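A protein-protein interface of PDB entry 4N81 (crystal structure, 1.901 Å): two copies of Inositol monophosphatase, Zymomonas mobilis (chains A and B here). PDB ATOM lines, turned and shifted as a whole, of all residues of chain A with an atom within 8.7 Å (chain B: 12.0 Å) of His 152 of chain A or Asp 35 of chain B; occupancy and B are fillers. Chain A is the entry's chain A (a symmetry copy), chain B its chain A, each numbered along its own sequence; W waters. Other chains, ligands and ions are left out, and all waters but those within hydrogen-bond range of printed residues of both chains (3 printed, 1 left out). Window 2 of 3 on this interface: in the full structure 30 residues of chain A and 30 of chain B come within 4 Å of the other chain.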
ATOM      1  N   ARG A 145      -2.534 -29.144 -12.913  1.00  0.00           N
ATOM      2  CA  ARG A 145      -1.287 -29.210 -13.679  1.00  0.00           C
ATOM      3  C   ARG A 145      -0.780 -27.859 -14.058  1.00  0.00           C
ATOM      4  O   ARG A 145      -1.530 -26.852 -14.050  1.00  0.00           O
ATOM      5  CB  ARG A 145      -1.464 -30.031 -14.948  1.00  0.00           C
ATOM      6  CG  ARG A 145      -2.384 -29.337 -16.020  1.00  0.00           C
ATOM      7  CD  ARG A 145      -2.546 -30.310 -17.229  1.00  0.00           C
ATOM      8  NE  ARG A 145      -3.415 -29.701 -18.246  1.00  0.00           N
ATOM      9  CZ  ARG A 145      -4.155 -30.413 -19.098  1.00  0.00           C
ATOM     10  NH1 ARG A 145      -4.036 -31.743 -19.128  1.00  0.00           N
ATOM     11  NH2 ARG A 145      -4.941 -29.772 -19.968  1.00  0.00           N
ATOM     12  N   SER A 146       0.517 -27.810 -14.362  1.00  0.00           N
ATOM     13  CA  SER A 146       1.096 -26.567 -14.843  1.00  0.00           C
ATOM     14  C   SER A 146       0.874 -26.454 -16.358  1.00  0.00           C
ATOM     15  O   SER A 146       0.560 -27.434 -17.027  1.00  0.00           O
ATOM     16  CB  SER A 146       2.593 -26.491 -14.561  1.00  0.00           C
ATOM     17  OG  SER A 146       3.204 -27.580 -15.223  1.00  0.00           O
ATOM     18  N   CYS A 147       1.068 -25.251 -16.899  1.00  0.00           N
ATOM     19  CA  CYS A 147       0.803 -25.027 -18.320  1.00  0.00           C
ATOM     20  C   CYS A 147       1.681 -23.854 -18.797  1.00  0.00           C
ATOM     21  O   CYS A 147       1.718 -22.807 -18.159  1.00  0.00           O
ATOM     22  CB  CYS A 147      -0.681 -24.657 -18.503  1.00  0.00           C
ATOM     23  SG  CYS A 147      -1.073 -24.488 -20.290  1.00  0.00           S
ATOM     24  N   PRO A 148       2.538 -24.105 -19.772  1.00  0.00           N
ATOM     25  CA  PRO A 148       3.525 -23.082 -20.179  1.00  0.00           C
ATOM     26  C   PRO A 148       2.963 -21.749 -20.709  1.00  0.00           C
ATOM     27  O   PRO A 148       3.576 -20.708 -20.507  1.00  0.00           O
ATOM     28  CB  PRO A 148       4.390 -23.820 -21.203  1.00  0.00           C
ATOM     29  CG  PRO A 148       3.472 -24.793 -21.847  1.00  0.00           C
ATOM     30  CD  PRO A 148       2.558 -25.266 -20.672  1.00  0.00           C
ATOM     31  N   ALA A 149       1.824 -21.800 -21.415  1.00  0.00           N
ATOM     32  CA  ALA A 149       1.362 -20.636 -22.195  1.00  0.00           C
ATOM     33  C   ALA A 149      -0.056 -20.933 -22.672  1.00  0.00           C
ATOM     34  O   ALA A 149      -0.428 -22.104 -22.787  1.00  0.00           O
ATOM     35  CB  ALA A 149       2.263 -20.414 -23.440  1.00  0.00           C
ATOM     36  N   LEU A 150      -0.795 -19.898 -23.088  1.00  0.00           N
ATOM     37  CA  LEU A 150      -2.158 -20.114 -23.594  1.00  0.00           C
ATOM     38  C   LEU A 150      -2.234 -21.020 -24.783  1.00  0.00           C
ATOM     39  O   LEU A 150      -3.166 -21.797 -24.896  1.00  0.00           O
ATOM     40  CB  LEU A 150      -2.767 -18.788 -24.033  1.00  0.00           C
ATOM     41  CG  LEU A 150      -2.996 -17.799 -22.911  1.00  0.00           C
ATOM     42  CD1 LEU A 150      -3.711 -16.523 -23.523  1.00  0.00           C
ATOM     43  CD2 LEU A 150      -3.878 -18.448 -21.830  1.00  0.00           C
ATOM     44  N   ASP A 151      -1.212 -20.996 -25.636  1.00  0.00           N
ATOM     45  CA  ASP A 151      -1.309 -21.812 -26.842  1.00  0.00           C
ATOM     46  C   ASP A 151      -1.150 -23.312 -26.547  1.00  0.00           C
ATOM     47  O   ASP A 151      -1.248 -24.139 -27.453  1.00  0.00           O
ATOM     48  CB  ASP A 151      -0.407 -21.315 -27.983  1.00  0.00           C
ATOM     49  CG  ASP A 151       1.082 -21.352 -27.645  1.00  0.00           C
ATOM     50  OD1 ASP A 151       1.493 -21.892 -26.598  1.00  0.00           O
ATOM     51  OD2 ASP A 151       1.865 -20.822 -28.458  1.00  0.00           O
ATOM     52  N   HIS A 152      -0.850 -23.657 -25.292  1.00  0.00           N
ATOM     53  CA  HIS A 152      -0.900 -25.054 -24.829  1.00  0.00           C
ATOM     54  C   HIS A 152      -2.082 -25.380 -23.945  1.00  0.00           C
ATOM     55  O   HIS A 152      -2.289 -26.557 -23.533  1.00  0.00           O
ATOM     56  CB  HIS A 152       0.395 -25.446 -24.093  1.00  0.00           C
ATOM     57  CG  HIS A 152       1.588 -25.533 -24.992  1.00  0.00           C
ATOM     58  ND1 HIS A 152       1.851 -26.629 -25.781  1.00  0.00           N
ATOM     59  CD2 HIS A 152       2.567 -24.639 -25.246  1.00  0.00           C
ATOM     60  CE1 HIS A 152       2.941 -26.396 -26.493  1.00  0.00           C
ATOM     61  NE2 HIS A 152       3.411 -25.204 -26.164  1.00  0.00           N
ATOM     62  N   ALA A 153      -2.872 -24.360 -23.626  1.00  0.00           N
ATOM     63  CA  ALA A 153      -3.914 -24.526 -22.617  1.00  0.00           C
ATOM     64  C   ALA A 153      -5.249 -25.071 -23.188  1.00  0.00           C
ATOM     65  O   ALA A 153      -5.666 -24.702 -24.288  1.00  0.00           O
ATOM     66  CB  ALA A 153      -4.171 -23.196 -21.903  1.00  0.00           C
ATOM     67  N   LEU A 154      -5.903 -25.920 -22.400  1.00  0.00           N
ATOM     68  CA  LEU A 154      -7.283 -26.310 -22.669  1.00  0.00           C
ATOM     69  C   LEU A 154      -8.216 -25.433 -21.845  1.00  0.00           C
ATOM     70  O   LEU A 154      -8.070 -25.353 -20.639  1.00  0.00           O
ATOM     71  CB  LEU A 154      -7.495 -27.759 -22.259  1.00  0.00           C
ATOM     72  CG  LEU A 154      -8.875 -28.351 -22.444  1.00  0.00           C
ATOM     73  CD1 LEU A 154      -9.334 -28.111 -23.852  1.00  0.00           C
ATOM     74  CD2 LEU A 154      -8.709 -29.884 -22.268  1.00  0.00           C
ATOM     75  N   LEU A 155      -9.150 -24.762 -22.538  1.00  0.00           N
ATOM     76  CA  LEU A 155     -10.062 -23.792 -21.941  1.00  0.00           C
ATOM     77  C   LEU A 155     -11.444 -24.469 -21.943  1.00  0.00           C
ATOM     78  O   LEU A 155     -11.757 -25.177 -22.878  1.00  0.00           O
ATOM     79  CB  LEU A 155     -10.158 -22.569 -22.869  1.00  0.00           C
ATOM     80  CG  LEU A 155     -11.219 -21.468 -22.599  1.00  0.00           C
ATOM     81  CD1 LEU A 155     -10.982 -20.791 -21.224  1.00  0.00           C
ATOM     82  CD2 LEU A 155     -11.125 -20.424 -23.765  1.00  0.00           C
ATOM     83  N   LYS A 177      -6.833 -17.817 -28.603  1.00  0.00           N
ATOM     84  CA  LYS A 177      -5.435 -17.913 -28.181  1.00  0.00           C
ATOM     85  C   LYS A 177      -5.092 -19.230 -27.481  1.00  0.00           C
ATOM     86  O   LYS A 177      -3.883 -19.520 -27.238  1.00  0.00           O
ATOM     87  CB  LYS A 177      -5.091 -16.742 -27.236  1.00  0.00           C
ATOM     88  CG  LYS A 177      -5.091 -15.395 -27.895  1.00  0.00           C
ATOM     89  CD  LYS A 177      -4.026 -15.319 -28.956  1.00  0.00           C
ATOM     90  CE  LYS A 177      -3.903 -13.881 -29.537  1.00  0.00           C
ATOM     91  NZ  LYS A 177      -4.165 -12.825 -28.514  1.00  0.00           N
ATOM     92  N   CYS A 178      -6.122 -20.030 -27.155  1.00  0.00           N
ATOM     93  CA  CYS A 178      -5.912 -21.338 -26.481  1.00  0.00           C
ATOM     94  C   CYS A 178      -5.757 -22.491 -27.451  1.00  0.00           C
ATOM     95  O   CYS A 178      -6.108 -22.361 -28.631  1.00  0.00           O
ATOM     96  CB  CYS A 178      -7.024 -21.653 -25.476  1.00  0.00           C
ATOM     97  SG  CYS A 178      -6.971 -20.404 -24.081  1.00  0.00           S
ATOM     98  N   ARG A 179      -5.189 -23.597 -26.975  1.00  0.00           N
ATOM     99  CA  ARG A 179      -4.961 -24.770 -27.822  1.00  0.00           C
ATOM    100  C   ARG A 179      -6.301 -25.451 -28.184  1.00  0.00           C
ATOM    101  O   ARG A 179      -6.487 -25.937 -29.288  1.00  0.00           O
ATOM    102  CB  ARG A 179      -4.146 -25.805 -27.034  1.00  0.00           C
ATOM    103  CG  ARG A 179      -3.766 -27.070 -27.885  1.00  0.00           C
ATOM    104  CD  ARG A 179      -4.331 -28.395 -27.272  1.00  0.00           C
ATOM    105  NE  ARG A 179      -3.290 -29.221 -26.638  1.00  0.00           N
ATOM    106  CZ  ARG A 179      -3.281 -30.559 -26.548  1.00  0.00           C
ATOM    107  NH1 ARG A 179      -4.252 -31.302 -27.047  1.00  0.00           N
ATOM    108  NH2 ARG A 179      -2.260 -31.163 -25.961  1.00  0.00           N
ATOM    109  N   ASP A 180      -7.203 -25.540 -27.225  1.00  0.00           N
ATOM    110  CA  ASP A 180      -8.521 -26.121 -27.516  1.00  0.00           C
ATOM    111  C   ASP A 180      -9.517 -25.636 -26.518  1.00  0.00           C
ATOM    112  O   ASP A 180      -9.118 -25.225 -25.436  1.00  0.00           O
ATOM    113  CB  ASP A 180      -8.540 -27.638 -27.408  1.00  0.00           C
ATOM    114  CG  ASP A 180      -9.823 -28.232 -28.070  1.00  0.00           C
ATOM    115  OD1 ASP A 180     -10.334 -27.617 -29.060  1.00  0.00           O
ATOM    116  OD2 ASP A 180     -10.347 -29.260 -27.582  1.00  0.00           O
ATOM    117  N   CYS A 198      -7.833 -29.834 -17.190  1.00  0.00           N
ATOM    118  CA  CYS A 198      -8.320 -28.652 -17.885  1.00  0.00           C
ATOM    119  C   CYS A 198      -7.402 -27.507 -17.391  1.00  0.00           C
ATOM    120  O   CYS A 198      -6.982 -27.589 -16.240  1.00  0.00           O
ATOM    121  CB  CYS A 198      -9.810 -28.368 -17.376  1.00  0.00           C
ATOM    122  SG  CYS A 198     -10.495 -27.087 -18.254  1.00  0.00           S
ATOM    123  N   ASP A 199      -7.101 -26.457 -18.183  1.00  0.00           N
ATOM    124  CA  ASP A 199      -6.189 -25.411 -17.649  1.00  0.00           C
ATOM    125  C   ASP A 199      -6.864 -24.120 -17.278  1.00  0.00           C
ATOM    126  O   ASP A 199      -6.375 -23.409 -16.401  1.00  0.00           O
ATOM    127  CB  ASP A 199      -5.094 -25.090 -18.684  1.00  0.00           C
ATOM    128  CG  ASP A 199      -4.288 -26.351 -19.054  1.00  0.00           C
ATOM    129  OD1 ASP A 199      -4.430 -26.871 -20.174  1.00  0.00           O
ATOM    130  OD2 ASP A 199      -3.616 -26.887 -18.141  1.00  0.00           O
ATOM    131  N   LEU A 200      -7.947 -23.784 -17.984  1.00  0.00           N
ATOM    132  CA  LEU A 200      -8.668 -22.525 -17.714  1.00  0.00           C
ATOM    133  C   LEU A 200     -10.164 -22.782 -17.808  1.00  0.00           C
ATOM    134  O   LEU A 200     -10.609 -23.550 -18.661  1.00  0.00           O
ATOM    135  CB  LEU A 200      -8.302 -21.482 -18.818  1.00  0.00           C
ATOM    136  CG  LEU A 200      -6.855 -20.969 -18.721  1.00  0.00           C
ATOM    137  CD1 LEU A 200      -6.448 -20.198 -20.027  1.00  0.00           C
ATOM    138  CD2 LEU A 200      -6.661 -20.032 -17.534  1.00  0.00           C
ATOM    139  N   LEU A 249      -0.721 -18.530 -15.537  1.00  0.00           N
ATOM    140  CA  LEU A 249      -1.564 -18.277 -16.695  1.00  0.00           C
ATOM    141  C   LEU A 249      -2.641 -17.241 -16.438  1.00  0.00           C
ATOM    142  O   LEU A 249      -3.324 -16.828 -17.391  1.00  0.00           O
ATOM    143  CB  LEU A 249      -2.237 -19.590 -17.196  1.00  0.00           C
ATOM    144  CG  LEU A 249      -1.804 -20.013 -18.604  1.00  0.00           C
ATOM    145  CD1 LEU A 249      -0.314 -19.891 -18.800  1.00  0.00           C
ATOM    146  CD2 LEU A 249      -2.271 -21.425 -18.900  1.00  0.00           C
ATOM    147  N   PRO B  31      -1.943 -38.567 -17.202  1.00  0.00           N
ATOM    148  CA  PRO B  31      -1.260 -37.262 -17.348  1.00  0.00           C
ATOM    149  C   PRO B  31      -0.996 -36.956 -18.827  1.00  0.00           C
ATOM    150  O   PRO B  31      -0.812 -37.881 -19.610  1.00  0.00           O
ATOM    151  CB  PRO B  31       0.095 -37.491 -16.640  1.00  0.00           C
ATOM    152  CG  PRO B  31      -0.151 -38.617 -15.710  1.00  0.00           C
ATOM    153  CD  PRO B  31      -1.177 -39.525 -16.370  1.00  0.00           C
ATOM    154  N   LEU B  32      -1.031 -35.692 -19.230  1.00  0.00           N
ATOM    155  CA  LEU B  32      -0.872 -35.344 -20.646  1.00  0.00           C
ATOM    156  C   LEU B  32       0.462 -34.667 -20.937  1.00  0.00           C
ATOM    157  O   LEU B  32       0.749 -33.590 -20.437  1.00  0.00           O
ATOM    158  CB  LEU B  32      -2.058 -34.449 -21.091  1.00  0.00           C
ATOM    159  CG  LEU B  32      -1.993 -33.850 -22.468  1.00  0.00           C
ATOM    160  CD1 LEU B  32      -1.895 -34.949 -23.590  1.00  0.00           C
ATOM    161  CD2 LEU B  32      -3.249 -32.995 -22.680  1.00  0.00           C
ATOM    162  N   THR B  33       1.308 -35.345 -21.692  1.00  0.00           N
ATOM    163  CA  THR B  33       2.618 -34.811 -22.027  1.00  0.00           C
ATOM    164  C   THR B  33       2.459 -33.788 -23.149  1.00  0.00           C
ATOM    165  O   THR B  33       1.645 -33.992 -24.045  1.00  0.00           O
ATOM    166  CB  THR B  33       3.532 -35.968 -22.465  1.00  0.00           C
ATOM    167  OG1 THR B  33       3.702 -36.847 -21.347  1.00  0.00           O
ATOM    168  CG2 THR B  33       4.963 -35.460 -22.913  1.00  0.00           C
ATOM    169  N   ILE B  34       3.262 -32.728 -23.144  1.00  0.00           N
ATOM    170  CA  ILE B  34       3.135 -31.731 -24.202  1.00  0.00           C
ATOM    171  C   ILE B  34       4.472 -31.352 -24.808  1.00  0.00           C
ATOM    172  O   ILE B  34       5.498 -31.644 -24.253  1.00  0.00           O
ATOM    173  CB  ILE B  34       2.521 -30.434 -23.686  1.00  0.00           C
ATOM    174  CG1 ILE B  34       3.372 -29.902 -22.522  1.00  0.00           C
ATOM    175  CG2 ILE B  34       1.040 -30.678 -23.353  1.00  0.00           C
ATOM    176  CD1 ILE B  34       2.866 -28.579 -21.974  1.00  0.00           C
ATOM    177  N   ASP B  35       4.396 -30.737 -25.986  1.00  0.00           N
ATOM    178  CA  ASP B  35       5.456 -29.920 -26.568  1.00  0.00           C
ATOM    179  C   ASP B  35       6.738 -30.692 -26.811  1.00  0.00           C
ATOM    180  O   ASP B  35       7.840 -30.159 -26.623  1.00  0.00           O
ATOM    181  CB  ASP B  35       5.763 -28.699 -25.667  1.00  0.00           C
ATOM    182  CG  ASP B  35       6.525 -27.648 -26.385  1.00  0.00           C
ATOM    183  OD1 ASP B  35       7.507 -27.072 -25.822  1.00  0.00           O
ATOM    184  OD2 ASP B  35       6.194 -27.464 -27.574  1.00  0.00           O
ATOM    185  N   LEU B  36       6.590 -31.945 -27.240  1.00  0.00           N
ATOM    186  CA  LEU B  36       7.777 -32.770 -27.576  1.00  0.00           C
ATOM    187  C   LEU B  36       7.907 -32.958 -29.088  1.00  0.00           C
ATOM    188  O   LEU B  36       6.944 -32.742 -29.815  1.00  0.00           O
ATOM    189  CB  LEU B  36       7.680 -34.153 -26.893  1.00  0.00           C
ATOM    190  CG  LEU B  36       8.029 -34.181 -25.393  1.00  0.00           C
ATOM    191  CD1 LEU B  36       8.019 -35.610 -24.867  1.00  0.00           C
ATOM    192  CD2 LEU B  36       9.417 -33.565 -25.130  1.00  0.00           C
ATOM    193  N   LYS B  37       9.095 -33.378 -29.541  1.00  0.00           N
ATOM    194  CA  LYS B  37       9.304 -33.648 -30.968  1.00  0.00           C
ATOM    195  C   LYS B  37       8.415 -34.791 -31.469  1.00  0.00           C
ATOM    196  O   LYS B  37       8.137 -34.867 -32.655  1.00  0.00           O
ATOM    197  CB  LYS B  37      10.786 -33.906 -31.291  1.00  0.00           C
ATOM    198  CG  LYS B  37      11.349 -35.207 -30.731  1.00  0.00           C
ATOM    199  CD  LYS B  37      12.768 -35.503 -31.284  1.00  0.00           C
ATOM    200  CE  LYS B  37      13.759 -35.837 -30.160  1.00  0.00           C
ATOM    201  NZ  LYS B  37      14.701 -34.695 -29.743  1.00  0.00           N
ATOM    202  N   ALA B  38       7.968 -35.670 -30.565  1.00  0.00           N
ATOM    203  CA  ALA B  38       7.034 -36.740 -30.929  1.00  0.00           C
ATOM    204  C   ALA B  38       5.800 -36.660 -30.055  1.00  0.00           C
ATOM    205  O   ALA B  38       5.790 -35.904 -29.082  1.00  0.00           O
ATOM    206  CB  ALA B  38       7.704 -38.091 -30.781  1.00  0.00           C
ATOM    207  N   ASP B  39       4.766 -37.428 -30.424  1.00  0.00           N
ATOM    208  CA  ASP B  39       3.464 -37.481 -29.759  1.00  0.00           C
ATOM    209  C   ASP B  39       3.447 -38.563 -28.679  1.00  0.00           C
ATOM    210  O   ASP B  39       3.367 -39.779 -28.950  1.00  0.00           O
ATOM    211  CB  ASP B  39       2.357 -37.731 -30.815  1.00  0.00           C
ATOM    212  CG  ASP B  39       0.952 -37.839 -30.222  1.00  0.00           C
ATOM    213  OD1 ASP B  39       0.740 -37.636 -28.999  1.00  0.00           O
ATOM    214  OD2 ASP B  39       0.009 -38.099 -31.009  1.00  0.00           O
ATOM    215  N   HIS B  40       3.511 -38.108 -27.437  1.00  0.00           N
ATOM    216  CA  HIS B  40       3.495 -39.003 -26.284  1.00  0.00           C
ATOM    217  C   HIS B  40       2.094 -39.062 -25.670  1.00  0.00           C
ATOM    218  O   HIS B  40       1.940 -39.443 -24.501  1.00  0.00           O
ATOM    219  CB  HIS B  40       4.478 -38.472 -25.264  1.00  0.00           C
ATOM    220  CG  HIS B  40       5.913 -38.729 -25.624  1.00  0.00           C
ATOM    221  ND1 HIS B  40       6.811 -39.265 -24.725  1.00  0.00           N
ATOM    222  CD2 HIS B  40       6.594 -38.562 -26.788  1.00  0.00           C
ATOM    223  CE1 HIS B  40       8.006 -39.359 -25.300  1.00  0.00           C
ATOM    224  NE2 HIS B  40       7.898 -38.947 -26.553  1.00  0.00           N
ATOM    225  N   SER B  41       1.076 -38.598 -26.390  1.00  0.00           N
ATOM    226  CA  SER B  41      -0.257 -38.492 -25.756  1.00  0.00           C
ATOM    227  C   SER B  41      -0.944 -39.859 -25.506  1.00  0.00           C
ATOM    228  O   SER B  41      -0.870 -40.771 -26.336  1.00  0.00           O
ATOM    229  CB  SER B  41      -1.196 -37.590 -26.568  1.00  0.00           C
ATOM    230  OG  SER B  41      -1.587 -38.271 -27.742  1.00  0.00           O
ATOM    231  N   PRO B  42      -1.633 -39.990 -24.353  1.00  0.00           N
ATOM    232  CA  PRO B  42      -2.412 -41.209 -24.060  1.00  0.00           C
ATOM    233  C   PRO B  42      -3.497 -41.504 -25.102  1.00  0.00           C
ATOM    234  O   PRO B  42      -3.757 -42.693 -25.392  1.00  0.00           O
ATOM    235  CB  PRO B  42      -3.088 -40.890 -22.710  1.00  0.00           C
ATOM    236  CG  PRO B  42      -2.212 -39.847 -22.076  1.00  0.00           C
ATOM    237  CD  PRO B  42      -1.650 -39.021 -23.235  1.00  0.00           C
ATOM    238  N   THR B  44      -3.494 -41.025 -28.305  1.00  0.00           N
ATOM    239  CA  THR B  44      -2.908 -41.633 -29.474  1.00  0.00           C
ATOM    240  C   THR B  44      -2.534 -43.090 -29.204  1.00  0.00           C
ATOM    241  O   THR B  44      -2.790 -43.982 -30.053  1.00  0.00           O
ATOM    242  CB  THR B  44      -1.647 -40.810 -29.919  1.00  0.00           C
ATOM    243  OG1 THR B  44      -2.095 -39.504 -30.333  1.00  0.00           O
ATOM    244  CG2 THR B  44      -0.967 -41.495 -31.056  1.00  0.00           C
ATOM    245  N   ARG B  92     -11.209 -34.956 -28.543  1.00  0.00           N
ATOM    246  CA  ARG B  92     -10.917 -33.806 -27.657  1.00  0.00           C
ATOM    247  C   ARG B  92     -11.538 -33.934 -26.251  1.00  0.00           C
ATOM    248  O   ARG B  92     -10.890 -33.568 -25.242  1.00  0.00           O
ATOM    249  CB  ARG B  92     -11.385 -32.514 -28.362  1.00  0.00           C
ATOM    250  CG  ARG B  92     -10.634 -32.336 -29.700  1.00  0.00           C
ATOM    251  CD  ARG B  92     -10.374 -30.895 -30.106  1.00  0.00           C
ATOM    252  NE  ARG B  92     -11.538 -30.214 -30.664  1.00  0.00           N
ATOM    253  CZ  ARG B  92     -12.446 -29.550 -29.948  1.00  0.00           C
ATOM    254  NH1 ARG B  92     -12.398 -29.527 -28.613  1.00  0.00           N
ATOM    255  NH2 ARG B  92     -13.461 -28.950 -30.563  1.00  0.00           N
ATOM    256  N   ILE B  95      -9.330 -36.193 -24.348  1.00  0.00           N
ATOM    257  CA  ILE B  95      -8.089 -35.502 -23.956  1.00  0.00           C
ATOM    258  C   ILE B  95      -8.365 -34.640 -22.726  1.00  0.00           C
ATOM    259  O   ILE B  95      -7.525 -34.534 -21.803  1.00  0.00           O
ATOM    260  CB  ILE B  95      -7.585 -34.627 -25.119  1.00  0.00           C
ATOM    261  CG1 ILE B  95      -6.885 -35.520 -26.161  1.00  0.00           C
ATOM    262  CG2 ILE B  95      -6.576 -33.534 -24.644  1.00  0.00           C
ATOM    263  CD1 ILE B  95      -6.706 -34.812 -27.519  1.00  0.00           C
ATOM    264  N   GLY B  96      -9.596 -34.147 -22.659  1.00  0.00           N
ATOM    265  CA  GLY B  96     -10.021 -33.330 -21.516  1.00  0.00           C
ATOM    266  C   GLY B  96     -10.514 -34.135 -20.313  1.00  0.00           C
ATOM    267  O   GLY B  96     -10.993 -33.566 -19.316  1.00  0.00           O
HETATM  268  O   HOH W   1      -6.344 -32.461 -20.578  1.00  0.00           O
HETATM  269  O   HOH W   2       0.226 -33.131 -26.194  1.00  0.00           O
HETATM  270  O   HOH W   3      -9.072 -31.302 -25.865  1.00  0.00           O
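Water W1 lies within hydrogen-bond range of O of Ile 95 of chain B (2.7 Å) and NH1 of Arg 145 of chain A (2.8 Å).
Water W2 lies within hydrogen-bond range of O of Thr 33 of chain B (2.7 Å) and NH2 of Arg 179 of chain A (3.2 Å).
Water W3 bridges OD2 of Asp 180 of chain A and O of Arg 92 of chain B.
Of the printed residues of chain B, Arg 145 of chain A touches Leu 32.
Cys 147 of chain A touches none of the printed residues of chain B.
Ala 149 of chain A touches none of the printed residues of chain B.
His 152 of chain A touches just one residue of chain B: Asp 35.
No residue of chain B comes within 4 Å of Ala 153 of chain A.
Of chain B, only Gly 96 comes within 4 Å of Leu 154 of chain A.
No residue of chain B comes within 4 Å of Cys 178 of chain A.
Of the printed residues of chain B, Arg 179 of chain A touches Leu 32 (3.9 Å).
Leu 249 of chain A touches none of the printed residues of chain B.
Printed residues of chain A within 4 Å of Arg 92 of chain B: Asp 180.
Of the printed residues of chain A, Gly 96 of chain B touches Leu 154 (3.8 Å).
The nearest residue of chain B that does not touch His 152 of chain A is Ile 34 of chain B (4.4 Å).
The nearest residue of chain A that does not touch Asp 35 of chain B is Pro 148 of chain A (5.9 Å).
Among the printed residues, merely in contact across the chains: Arg 145 of chain A with Leu 32 of chain B (3.8 Å), Pro 148 of chain A with Ile 34 of chain B (3.6 Å), His 152 of chain A with Asp 35 of chain B (3.6 Å), Leu 154 of chain A with Gly 96 of chain B (3.8 Å) and Arg 179 of chain A with Leu 32 of chain B (3.9 Å).
The side-chain carboxylate (OD1) of Asp 180 of chain A lies within salt-bridge range of the guanidinium group (NH1) of Arg 92 of chain B, at 2.8 Å.
No position is printed for both chains.
Of the 6 pairs that touch across the chains among the printed residues, none has its exchanged pair printed and touching as well.
Printed residues of chain A that touch a printed residue of chain B: Arg 145, Pro 148, His 152, Leu 154, Arg 179 and Asp 180.
Hydrophobic or aromatic side chains of chain A that line the printed part of chain B: Pro 148, His 152 and Leu 154.
Of the 16 printed residues of chain B, 5 touch a printed residue of chain A.
Hydrophobic or aromatic side chains of chain B that line the printed part of chain A: Leu 32 and Ile 34.
Among the printed residues, 6 pairs touch across the chains.
Among the printed residues, Asp or Glu carboxylates within 4 Å of a Lys or Arg side-chain nitrogen of the other chain: Asp 180 of chain A with Arg 92 of chain B.
The backbone carbonyl oxygen of Leu 150 of chain A sits at hydrogen-bond distance from the backbone NH of Arg 179 of chain A (3.4 Å).
O of Ala 153 of chain A is in hydrogen-bond range of N of Arg 179 of chain A (2.9 Å).
The backbone NH (N) of Asp 180 of chain A sits at hydrogen-bond distance from the backbone carbonyl oxygen (O) of Ala 153 of chain A (3.4 Å).
The backbone NH of Leu 154 of chain A is in hydrogen-bond range of the side-chain carboxylate of Asp 199 of chain A, at 2.8 Å.
The backbone carbonyl oxygen (O) of Leu 154 of chain A is in hydrogen-bond range of the backbone NH (N) of Leu 200 of chain A (3.1 Å).
The backbone NH (N) of Leu 155 of chain A sits at hydrogen-bond distance from the backbone carbonyl oxygen (O) of Asp 180 of chain A (2.9 Å).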
